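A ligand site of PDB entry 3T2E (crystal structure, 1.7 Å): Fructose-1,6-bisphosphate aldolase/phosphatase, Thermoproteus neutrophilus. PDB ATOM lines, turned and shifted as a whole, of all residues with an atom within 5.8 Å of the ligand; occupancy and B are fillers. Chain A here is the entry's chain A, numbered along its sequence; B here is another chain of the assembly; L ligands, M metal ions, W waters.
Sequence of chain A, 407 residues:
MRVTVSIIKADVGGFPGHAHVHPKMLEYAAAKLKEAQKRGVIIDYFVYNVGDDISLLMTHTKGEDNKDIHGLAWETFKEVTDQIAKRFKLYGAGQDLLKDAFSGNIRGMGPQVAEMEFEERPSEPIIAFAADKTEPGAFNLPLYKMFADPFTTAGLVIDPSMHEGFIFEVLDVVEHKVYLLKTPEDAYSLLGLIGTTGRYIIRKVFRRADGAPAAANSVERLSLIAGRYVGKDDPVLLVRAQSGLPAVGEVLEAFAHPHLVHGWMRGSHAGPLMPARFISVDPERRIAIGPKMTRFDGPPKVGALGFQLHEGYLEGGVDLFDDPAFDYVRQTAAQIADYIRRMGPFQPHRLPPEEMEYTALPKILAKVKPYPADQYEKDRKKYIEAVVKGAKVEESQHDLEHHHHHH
O3 of the ligand sits at hydrogen-bond distance from N of Arg 266, at 2.8 Å. OH of Tyr 91 lies within hydrogen-bond range of O7 of the ligand (2.6 Å). The side-chain amide oxygen of Gln 242 of chain B lies close to an oxygen (O9) of the ligand, 2.8 Å away. An oxygen (O3) of the ligand is in hydrogen-bond range of the side-chain carboxylate (OD2) of Asp 297 (2.6 Å). O8 of the ligand lies within salt-bridge range of NH1 of Arg 266, at 3.5 Å. An oxygen (O9) of the ligand sits at hydrogen-bond distance from the backbone NH (N) of Ser 243 of chain B (2.7 Å). O8 of the ligand sits at hydrogen-bond distance from OH of Tyr 358 (2.4 Å).
OD1 of Asp 297 sits at hydrogen-bond distance from N of Gly 249 of chain B. The backbone carbonyl oxygen (O) of Gly 267 lies within hydrogen-bond range of the backbone NH (N) of Glu 357, at 3.4 Å. The side-chain carboxylate (OE1) of Glu 250 of chain B sits at hydrogen-bond distance from the backbone NH (N) of Ala 247 of chain B (2.8 Å). The side-chain amide nitrogen (NE2) of Gln 242 of chain B lies close to the backbone NH (N) of Val 248 of chain B, at 2.9 Å. The side-chain hydroxyl of Tyr 91 lies within hydrogen-bond range of the backbone NH of Ser 243 of chain B, 3.5 Å away. The side-chain carboxylate (OD2) of Asp 159 of chain B lies within salt-bridge range of the guanidinium group (NH1) of Arg 266 (2.9 Å). The backbone carbonyl oxygen (O) of His 18 lies within hydrogen-bond range of the side-chain amino group (NZ) of Lys 133, 2.8 Å away. The backbone NH (N) of Met 265 sits close to the backbone carbonyl oxygen (O) of Phe 296.
Residues that only touch the ligand: His 18, Trp 264, Met 265, Gly 267, Asp 159 of chain B and Ala 247 of chain B. Within 4 Å of the ligand: His 18, Tyr 91, Trp 264, Met 265, Arg 266, Gly 267, Asp 297, Tyr 358, Asp 159 of chain B, Gln 242 of chain B, Ser 243 of chain B and Ala 247 of chain B.
Water W8 lies within hydrogen-bond range of an oxygen (O1) of the ligand and the side-chain carboxylate (OD1) of Asp 234. Water W9 lies within hydrogen-bond range of O7 of the ligand (2.6 Å) and NE2 of His 18 (2.8 Å). Water W4 lies within hydrogen-bond range of the side-chain carboxylate of Asp 159 of chain B (2.7 Å), an oxygen (O8) of the ligand (2.7 Å) and the backbone NH of Gly 244 of chain B (3.3 Å). Water W3 lies within hydrogen-bond range of O4 of the ligand (2.8 Å) and OH of Tyr 358 (2.9 Å). Water W7 lies within hydrogen-bond range of the backbone carbonyl oxygen of Trp 264 and an oxygen (O1) of the ligand. Water W2 lies within hydrogen-bond range of NE2 of Gln 242 of chain B (2.7 Å), N of His 18 (2.8 Å), OD1 of Asp 297 (2.9 Å) and O5 of the ligand (3.5 Å).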
ATOM      1  N   HIS A  18     -22.708 -14.598 -29.695  1.00  0.00           N
ATOM      2  CA  HIS A  18     -22.890 -15.917 -29.043  1.00  0.00           C
ATOM      3  C   HIS A  18     -24.383 -16.312 -28.994  1.00  0.00           C
ATOM      4  O   HIS A  18     -24.803 -17.082 -28.129  1.00  0.00           O
ATOM      5  CB  HIS A  18     -22.346 -15.852 -27.652  1.00  0.00           C
ATOM      6  CG  HIS A  18     -20.853 -15.571 -27.603  1.00  0.00           C
ATOM      7  ND1 HIS A  18     -19.918 -16.555 -27.844  1.00  0.00           N
ATOM      8  CD2 HIS A  18     -20.156 -14.457 -27.295  1.00  0.00           C
ATOM      9  CE1 HIS A  18     -18.706 -16.063 -27.726  1.00  0.00           C
ATOM     10  NE2 HIS A  18     -18.809 -14.786 -27.386  1.00  0.00           N
ATOM     11  N   ASP A  52     -25.316 -21.125 -28.769  1.00  0.00           N
ATOM     12  CA  ASP A  52     -24.149 -21.239 -29.668  1.00  0.00           C
ATOM     13  C   ASP A  52     -23.375 -22.527 -29.397  1.00  0.00           C
ATOM     14  O   ASP A  52     -22.216 -22.660 -29.885  1.00  0.00           O
ATOM     15  CB  ASP A  52     -23.159 -20.039 -29.508  1.00  0.00           C
ATOM     16  CG  ASP A  52     -22.660 -19.896 -28.062  1.00  0.00           C
ATOM     17  OD1 ASP A  52     -22.999 -20.673 -27.110  1.00  0.00           O
ATOM     18  OD2 ASP A  52     -21.825 -18.947 -27.772  1.00  0.00           O
ATOM     19  N   TYR A  91     -18.559 -15.662 -34.907  1.00  0.00           N
ATOM     20  CA  TYR A  91     -17.959 -15.090 -33.761  1.00  0.00           C
ATOM     21  C   TYR A  91     -17.490 -16.167 -32.787  1.00  0.00           C
ATOM     22  O   TYR A  91     -18.210 -17.078 -32.399  1.00  0.00           O
ATOM     23  CB  TYR A  91     -19.014 -14.098 -33.034  1.00  0.00           C
ATOM     24  CG  TYR A  91     -18.265 -13.220 -32.079  1.00  0.00           C
ATOM     25  CD1 TYR A  91     -17.511 -12.137 -32.540  1.00  0.00           C
ATOM     26  CD2 TYR A  91     -18.232 -13.514 -30.692  1.00  0.00           C
ATOM     27  CE1 TYR A  91     -16.706 -11.376 -31.699  1.00  0.00           C
ATOM     28  CE2 TYR A  91     -17.412 -12.755 -29.791  1.00  0.00           C
ATOM     29  CZ  TYR A  91     -16.666 -11.674 -30.343  1.00  0.00           C
ATOM     30  OH  TYR A  91     -15.854 -10.929 -29.537  1.00  0.00           O
ATOM     31  N   GLN A  95     -13.628 -21.343 -31.145  1.00  0.00           N
ATOM     32  CA  GLN A  95     -13.592 -20.961 -29.679  1.00  0.00           C
ATOM     33  C   GLN A  95     -13.074 -22.154 -28.797  1.00  0.00           C
ATOM     34  O   GLN A  95     -12.017 -22.077 -28.137  1.00  0.00           O
ATOM     35  CB  GLN A  95     -15.026 -20.402 -29.219  1.00  0.00           C
ATOM     36  CG  GLN A  95     -15.247 -19.933 -27.755  1.00  0.00           C
ATOM     37  CD  GLN A  95     -16.363 -18.839 -27.524  1.00  0.00           C
ATOM     38  OE1 GLN A  95     -17.482 -18.788 -28.155  1.00  0.00           O
ATOM     39  NE2 GLN A  95     -16.039 -17.943 -26.574  1.00  0.00           N
ATOM     40  N   LYS A 133     -24.971 -20.763 -21.831  1.00  0.00           N
ATOM     41  CA  LYS A 133     -24.734 -19.611 -20.961  1.00  0.00           C
ATOM     42  C   LYS A 133     -24.781 -19.955 -19.500  1.00  0.00           C
ATOM     43  O   LYS A 133     -25.293 -19.212 -18.637  1.00  0.00           O
ATOM     44  CB  LYS A 133     -25.763 -18.445 -21.283  1.00  0.00           C
ATOM     45  CG  LYS A 133     -25.809 -18.071 -22.810  1.00  0.00           C
ATOM     46  CD  LYS A 133     -24.487 -17.361 -23.174  1.00  0.00           C
ATOM     47  CE  LYS A 133     -24.490 -16.925 -24.631  1.00  0.00           C
ATOM     48  NZ  LYS A 133     -24.195 -18.070 -25.610  1.00  0.00           N
ATOM     49  N   ASP A 234     -20.183 -24.501 -21.138  1.00  0.00           N
ATOM     50  CA  ASP A 234     -21.673 -24.767 -21.069  1.00  0.00           C
ATOM     51  C   ASP A 234     -21.863 -26.307 -21.123  1.00  0.00           C
ATOM     52  O   ASP A 234     -21.211 -26.991 -21.974  1.00  0.00           O
ATOM     53  CB  ASP A 234     -22.345 -24.159 -22.282  1.00  0.00           C
ATOM     54  CG  ASP A 234     -22.154 -22.630 -22.391  1.00  0.00           C
ATOM     55  OD1 ASP A 234     -22.095 -22.025 -21.315  1.00  0.00           O
ATOM     56  OD2 ASP A 234     -21.976 -22.054 -23.474  1.00  0.00           O
ATOM     57  N   TRP A 264     -24.729 -16.604 -17.994  1.00  0.00           N
ATOM     58  CA  TRP A 264     -25.338 -15.442 -18.632  1.00  0.00           C
ATOM     59  C   TRP A 264     -24.245 -14.502 -19.149  1.00  0.00           C
ATOM     60  O   TRP A 264     -23.209 -14.992 -19.609  1.00  0.00           O
ATOM     61  CB  TRP A 264     -26.359 -14.749 -17.692  1.00  0.00           C
ATOM     62  CG  TRP A 264     -27.482 -14.056 -18.386  1.00  0.00           C
ATOM     63  CD1 TRP A 264     -27.691 -13.930 -19.752  1.00  0.00           C
ATOM     64  CD2 TRP A 264     -28.600 -13.462 -17.722  1.00  0.00           C
ATOM     65  NE1 TRP A 264     -28.923 -13.271 -19.948  1.00  0.00           N
ATOM     66  CE2 TRP A 264     -29.472 -12.969 -18.720  1.00  0.00           C
ATOM     67  CE3 TRP A 264     -28.911 -13.247 -16.338  1.00  0.00           C
ATOM     68  CZ2 TRP A 264     -30.698 -12.337 -18.409  1.00  0.00           C
ATOM     69  CZ3 TRP A 264     -30.141 -12.619 -16.014  1.00  0.00           C
ATOM     70  CH2 TRP A 264     -31.018 -12.127 -17.070  1.00  0.00           C
ATOM     71  N   MET A 265     -24.501 -13.194 -19.235  1.00  0.00           N
ATOM     72  CA  MET A 265     -23.540 -12.300 -19.947  1.00  0.00           C
ATOM     73  C   MET A 265     -22.121 -12.429 -19.343  1.00  0.00           C
ATOM     74  O   MET A 265     -21.916 -12.295 -18.132  1.00  0.00           O
ATOM     75  CB  MET A 265     -24.064 -10.873 -19.751  1.00  0.00           C
ATOM     76  CG  MET A 265     -23.094  -9.744 -20.290  1.00  0.00           C
ATOM     77  SD  MET A 265     -22.758  -9.872 -22.068  1.00  0.00           S
ATOM     78  CE  MET A 265     -24.453  -9.777 -22.790  1.00  0.00           C
ATOM     79  N   ARG A 266     -21.185 -12.606 -20.271  1.00  0.00           N
ATOM     80  CA  ARG A 266     -19.720 -12.579 -19.909  1.00  0.00           C
ATOM     81  C   ARG A 266     -19.378 -13.620 -18.876  1.00  0.00           C
ATOM     82  O   ARG A 266     -18.351 -13.529 -18.172  1.00  0.00           O
ATOM     83  CB  ARG A 266     -19.273 -11.161 -19.478  1.00  0.00           C
ATOM     84  CG  ARG A 266     -19.350 -10.235 -20.706  1.00  0.00           C
ATOM     85  CD  ARG A 266     -19.245  -8.758 -20.293  1.00  0.00           C
ATOM     86  NE  ARG A 266     -19.548  -7.883 -21.409  1.00  0.00           N
ATOM     87  CZ  ARG A 266     -18.664  -7.550 -22.371  1.00  0.00           C
ATOM     88  NH1 ARG A 266     -17.391  -8.116 -22.356  1.00  0.00           N
ATOM     89  NH2 ARG A 266     -19.045  -6.729 -23.343  1.00  0.00           N
ATOM     90  N   GLY A 267     -20.208 -14.672 -18.736  1.00  0.00           N
ATOM     91  CA  GLY A 267     -19.901 -15.742 -17.741  1.00  0.00           C
ATOM     92  C   GLY A 267     -19.845 -15.174 -16.323  1.00  0.00           C
ATOM     93  O   GLY A 267     -19.189 -15.756 -15.462  1.00  0.00           O
ATOM     94  N   PHE A 296     -29.199  -9.715 -22.961  1.00  0.00           N
ATOM     95  CA  PHE A 296     -28.088  -9.883 -22.053  1.00  0.00           C
ATOM     96  C   PHE A 296     -27.393 -11.236 -22.340  1.00  0.00           C
ATOM     97  O   PHE A 296     -26.800 -11.821 -21.445  1.00  0.00           O
ATOM     98  CB  PHE A 296     -28.552  -9.772 -20.585  1.00  0.00           C
ATOM     99  CG  PHE A 296     -27.474  -9.252 -19.645  1.00  0.00           C
ATOM    100  CD1 PHE A 296     -26.916  -7.971 -19.856  1.00  0.00           C
ATOM    101  CD2 PHE A 296     -27.103  -9.996 -18.519  1.00  0.00           C
ATOM    102  CE1 PHE A 296     -25.958  -7.459 -18.902  1.00  0.00           C
ATOM    103  CE2 PHE A 296     -26.174  -9.436 -17.549  1.00  0.00           C
ATOM    104  CZ  PHE A 296     -25.651  -8.134 -17.811  1.00  0.00           C
ATOM    105  N   ASP A 297     -27.450 -11.674 -23.605  1.00  0.00           N
ATOM    106  CA  ASP A 297     -26.837 -12.977 -24.065  1.00  0.00           C
ATOM    107  C   ASP A 297     -27.497 -14.171 -23.355  1.00  0.00           C
ATOM    108  O   ASP A 297     -26.842 -15.109 -22.956  1.00  0.00           O
ATOM    109  CB  ASP A 297     -25.250 -13.045 -23.859  1.00  0.00           C
ATOM    110  CG  ASP A 297     -24.503 -12.263 -24.921  1.00  0.00           C
ATOM    111  OD1 ASP A 297     -25.062 -11.800 -25.932  1.00  0.00           O
ATOM    112  OD2 ASP A 297     -23.252 -12.152 -24.652  1.00  0.00           O
ATOM    113  N   GLU A 357     -16.027 -14.612 -14.971  1.00  0.00           N
ATOM    114  CA  GLU A 357     -15.155 -14.876 -16.096  1.00  0.00           C
ATOM    115  C   GLU A 357     -14.430 -13.607 -16.582  1.00  0.00           C
ATOM    116  O   GLU A 357     -13.303 -13.688 -17.156  1.00  0.00           O
ATOM    117  CB  GLU A 357     -15.961 -15.518 -17.216  1.00  0.00           C
ATOM    118  CG  GLU A 357     -15.104 -15.730 -18.491  1.00  0.00           C
ATOM    119  CD  GLU A 357     -15.877 -16.289 -19.688  1.00  0.00           C
ATOM    120  OE1 GLU A 357     -16.929 -16.959 -19.490  1.00  0.00           O
ATOM    121  OE2 GLU A 357     -15.442 -16.021 -20.845  1.00  0.00           O
ATOM    122  N   TYR A 358     -15.089 -12.432 -16.407  1.00  0.00           N
ATOM    123  CA  TYR A 358     -14.536 -11.175 -16.844  1.00  0.00           C
ATOM    124  C   TYR A 358     -14.305 -10.389 -15.570  1.00  0.00           C
ATOM    125  O   TYR A 358     -15.228 -10.240 -14.784  1.00  0.00           O
ATOM    126  CB  TYR A 358     -15.573 -10.361 -17.755  1.00  0.00           C
ATOM    127  CG  TYR A 358     -15.545 -10.781 -19.247  1.00  0.00           C
ATOM    128  CD1 TYR A 358     -15.838 -12.107 -19.656  1.00  0.00           C
ATOM    129  CD2 TYR A 358     -15.301  -9.845 -20.225  1.00  0.00           C
ATOM    130  CE1 TYR A 358     -15.787 -12.456 -21.041  1.00  0.00           C
ATOM    131  CE2 TYR A 358     -15.155 -10.172 -21.523  1.00  0.00           C
ATOM    132  CZ  TYR A 358     -15.435 -11.444 -21.954  1.00  0.00           C
ATOM    133  OH  TYR A 358     -15.286 -11.617 -23.256  1.00  0.00           O
ATOM    134  N   ASP B 159     -15.202  -5.254 -18.375  1.00  0.00           N
ATOM    135  CA  ASP B 159     -14.424  -5.421 -19.564  1.00  0.00           C
ATOM    136  C   ASP B 159     -13.383  -4.349 -19.659  1.00  0.00           C
ATOM    137  O   ASP B 159     -13.658  -3.175 -20.057  1.00  0.00           O
ATOM    138  CB  ASP B 159     -15.242  -5.580 -20.843  1.00  0.00           C
ATOM    139  CG  ASP B 159     -14.441  -6.077 -22.064  1.00  0.00           C
ATOM    140  OD1 ASP B 159     -13.202  -6.017 -22.088  1.00  0.00           O
ATOM    141  OD2 ASP B 159     -15.028  -6.601 -23.005  1.00  0.00           O
ATOM    142  N   GLN B 242     -19.582  -6.588 -30.071  1.00  0.00           N
ATOM    143  CA  GLN B 242     -18.531  -7.459 -29.478  1.00  0.00           C
ATOM    144  C   GLN B 242     -17.083  -6.879 -29.566  1.00  0.00           C
ATOM    145  O   GLN B 242     -16.822  -5.842 -30.206  1.00  0.00           O
ATOM    146  CB  GLN B 242     -18.430  -8.846 -30.138  1.00  0.00           C
ATOM    147  CG  GLN B 242     -19.850  -9.561 -30.306  1.00  0.00           C
ATOM    148  CD  GLN B 242     -20.403 -10.112 -29.020  1.00  0.00           C
ATOM    149  OE1 GLN B 242     -19.686 -10.246 -27.951  1.00  0.00           O
ATOM    150  NE2 GLN B 242     -21.670 -10.444 -29.078  1.00  0.00           N
ATOM    151  N   SER B 243     -16.243  -7.551 -28.782  1.00  0.00           N
ATOM    152  CA  SER B 243     -14.773  -7.278 -28.847  1.00  0.00           C
ATOM    153  C   SER B 243     -14.462  -5.811 -28.544  1.00  0.00           C
ATOM    154  O   SER B 243     -13.833  -5.099 -29.363  1.00  0.00           O
ATOM    155  CB  SER B 243     -14.283  -7.774 -30.232  1.00  0.00           C
ATOM    156  OG  SER B 243     -12.840  -7.751 -30.220  1.00  0.00           O
ATOM    157  N   GLY B 244     -14.906  -5.336 -27.341  1.00  0.00           N
ATOM    158  CA  GLY B 244     -14.675  -3.908 -26.993  1.00  0.00           C
ATOM    159  C   GLY B 244     -15.830  -3.001 -27.377  1.00  0.00           C
ATOM    160  O   GLY B 244     -15.866  -1.883 -26.949  1.00  0.00           O
ATOM    161  N   LEU B 245     -16.799  -3.565 -28.085  1.00  0.00           N
ATOM    162  CA  LEU B 245     -18.077  -2.865 -28.398  1.00  0.00           C
ATOM    163  C   LEU B 245     -19.090  -3.750 -27.644  1.00  0.00           C
ATOM    164  O   LEU B 245     -18.811  -4.920 -27.259  1.00  0.00           O
ATOM    165  CB  LEU B 245     -18.371  -2.965 -29.880  1.00  0.00           C
ATOM    166  CG  LEU B 245     -17.293  -2.285 -30.715  1.00  0.00           C
ATOM    167  CD1 LEU B 245     -17.729  -2.437 -32.089  1.00  0.00           C
ATOM    168  CD2 LEU B 245     -17.177  -0.821 -30.351  1.00  0.00           C
ATOM    169  N   ALA B 247     -21.642  -6.348 -26.342  1.00  0.00           N
ATOM    170  CA  ALA B 247     -22.028  -7.688 -26.841  1.00  0.00           C
ATOM    171  C   ALA B 247     -23.365  -7.595 -27.535  1.00  0.00           C
ATOM    172  O   ALA B 247     -24.212  -6.696 -27.204  1.00  0.00           O
ATOM    173  CB  ALA B 247     -22.191  -8.636 -25.629  1.00  0.00           C
ATOM    174  N   VAL B 248     -23.680  -8.500 -28.447  1.00  0.00           N
ATOM    175  CA  VAL B 248     -25.040  -8.592 -29.037  1.00  0.00           C
ATOM    176  C   VAL B 248     -26.075  -8.537 -27.928  1.00  0.00           C
ATOM    177  O   VAL B 248     -27.058  -7.745 -28.078  1.00  0.00           O
ATOM    178  CB  VAL B 248     -25.171  -9.934 -29.787  1.00  0.00           C
ATOM    179  CG1 VAL B 248     -26.648 -10.234 -30.171  1.00  0.00           C
ATOM    180  CG2 VAL B 248     -24.306  -9.804 -31.174  1.00  0.00           C
ATOM    181  N   GLY B 249     -25.834  -9.226 -26.831  1.00  0.00           N
ATOM    182  CA  GLY B 249     -26.872  -9.233 -25.739  1.00  0.00           C
ATOM    183  C   GLY B 249     -26.960  -7.938 -25.023  1.00  0.00           C
ATOM    184  O   GLY B 249     -28.024  -7.658 -24.494  1.00  0.00           O
ATOM    185  N   GLU B 250     -25.891  -7.149 -24.948  1.00  0.00           N
ATOM    186  CA  GLU B 250     -25.927  -5.825 -24.291  1.00  0.00           C
ATOM    187  C   GLU B 250     -26.692  -4.825 -25.177  1.00  0.00           C
ATOM    188  O   GLU B 250     -27.516  -4.031 -24.681  1.00  0.00           O
ATOM    189  CB  GLU B 250     -24.478  -5.332 -23.968  1.00  0.00           C
ATOM    190  CG  GLU B 250     -23.929  -6.228 -22.804  1.00  0.00           C
ATOM    191  CD  GLU B 250     -22.397  -6.071 -22.544  1.00  0.00           C
ATOM    192  OE1 GLU B 250     -21.692  -5.834 -23.554  1.00  0.00           O
ATOM    193  OE2 GLU B 250     -21.976  -6.218 -21.394  1.00  0.00           O
HETATM  194  C1  LIG L   1     -20.657 -15.697 -22.161  1.00  0.00           C
HETATM  195  C2  LIG L   1     -20.413 -15.369 -23.429  1.00  0.00           C
HETATM  196  C3  LIG L   1     -20.840 -14.008 -23.899  1.00  0.00           C
HETATM  197  C4  LIG L   1     -19.592 -13.121 -24.124  1.00  0.00           C
HETATM  198  C5  LIG L   1     -19.951 -11.681 -24.494  1.00  0.00           C
HETATM  199  C6  LIG L   1     -18.776 -10.672 -24.657  1.00  0.00           C
HETATM  200  O1  LIG L   1     -20.208 -16.976 -21.882  1.00  0.00           O
HETATM  201  O2  LIG L   1     -19.738 -16.116 -24.201  1.00  0.00           O
HETATM  202  O3  LIG L   1     -21.775 -13.466 -22.894  1.00  0.00           O
HETATM  203  O4  LIG L   1     -18.778 -13.117 -22.954  1.00  0.00           O
HETATM  204  O5  LIG L   1     -20.793 -11.706 -25.650  1.00  0.00           O
HETATM  205  O6  LIG L   1     -17.930 -11.349 -25.640  1.00  0.00           O
HETATM  206  P1  LIG L   1     -16.702 -10.396 -26.146  1.00  0.00           P
HETATM  207  O7  LIG L   1     -15.875 -11.391 -26.997  1.00  0.00           O
HETATM  208  O8  LIG L   1     -15.934  -9.981 -24.928  1.00  0.00           O
HETATM  209  O9  LIG L   1     -17.235  -9.276 -26.974  1.00  0.00           O
HETATM  210 MG    MG M   1     -19.875 -18.646 -28.010  1.00  0.00          MG
HETATM  211  O   HOH W   1     -17.431  -6.717 -25.711  1.00  0.00           O
HETATM  212  O   HOH W   2     -23.233 -12.430 -28.049  1.00  0.00           O
HETATM  213  O   HOH W   3     -16.377 -14.251 -23.859  1.00  0.00           O
HETATM  214  O   HOH W   4     -14.329  -7.803 -25.276  1.00  0.00           O
HETATM  215  O   HOH W   5     -19.441 -18.838 -26.041  1.00  0.00           O
HETATM  216  O   HOH W   6     -13.230 -11.467 -26.876  1.00  0.00           O
HETATM  217  O   HOH W   7     -22.168 -17.655 -19.678  1.00  0.00           O
HETATM  218  O   HOH W   8     -21.402 -19.317 -22.025  1.00  0.00           O
HETATM  219  O   HOH W   9     -16.280 -13.969 -26.546  1.00  0.00           O
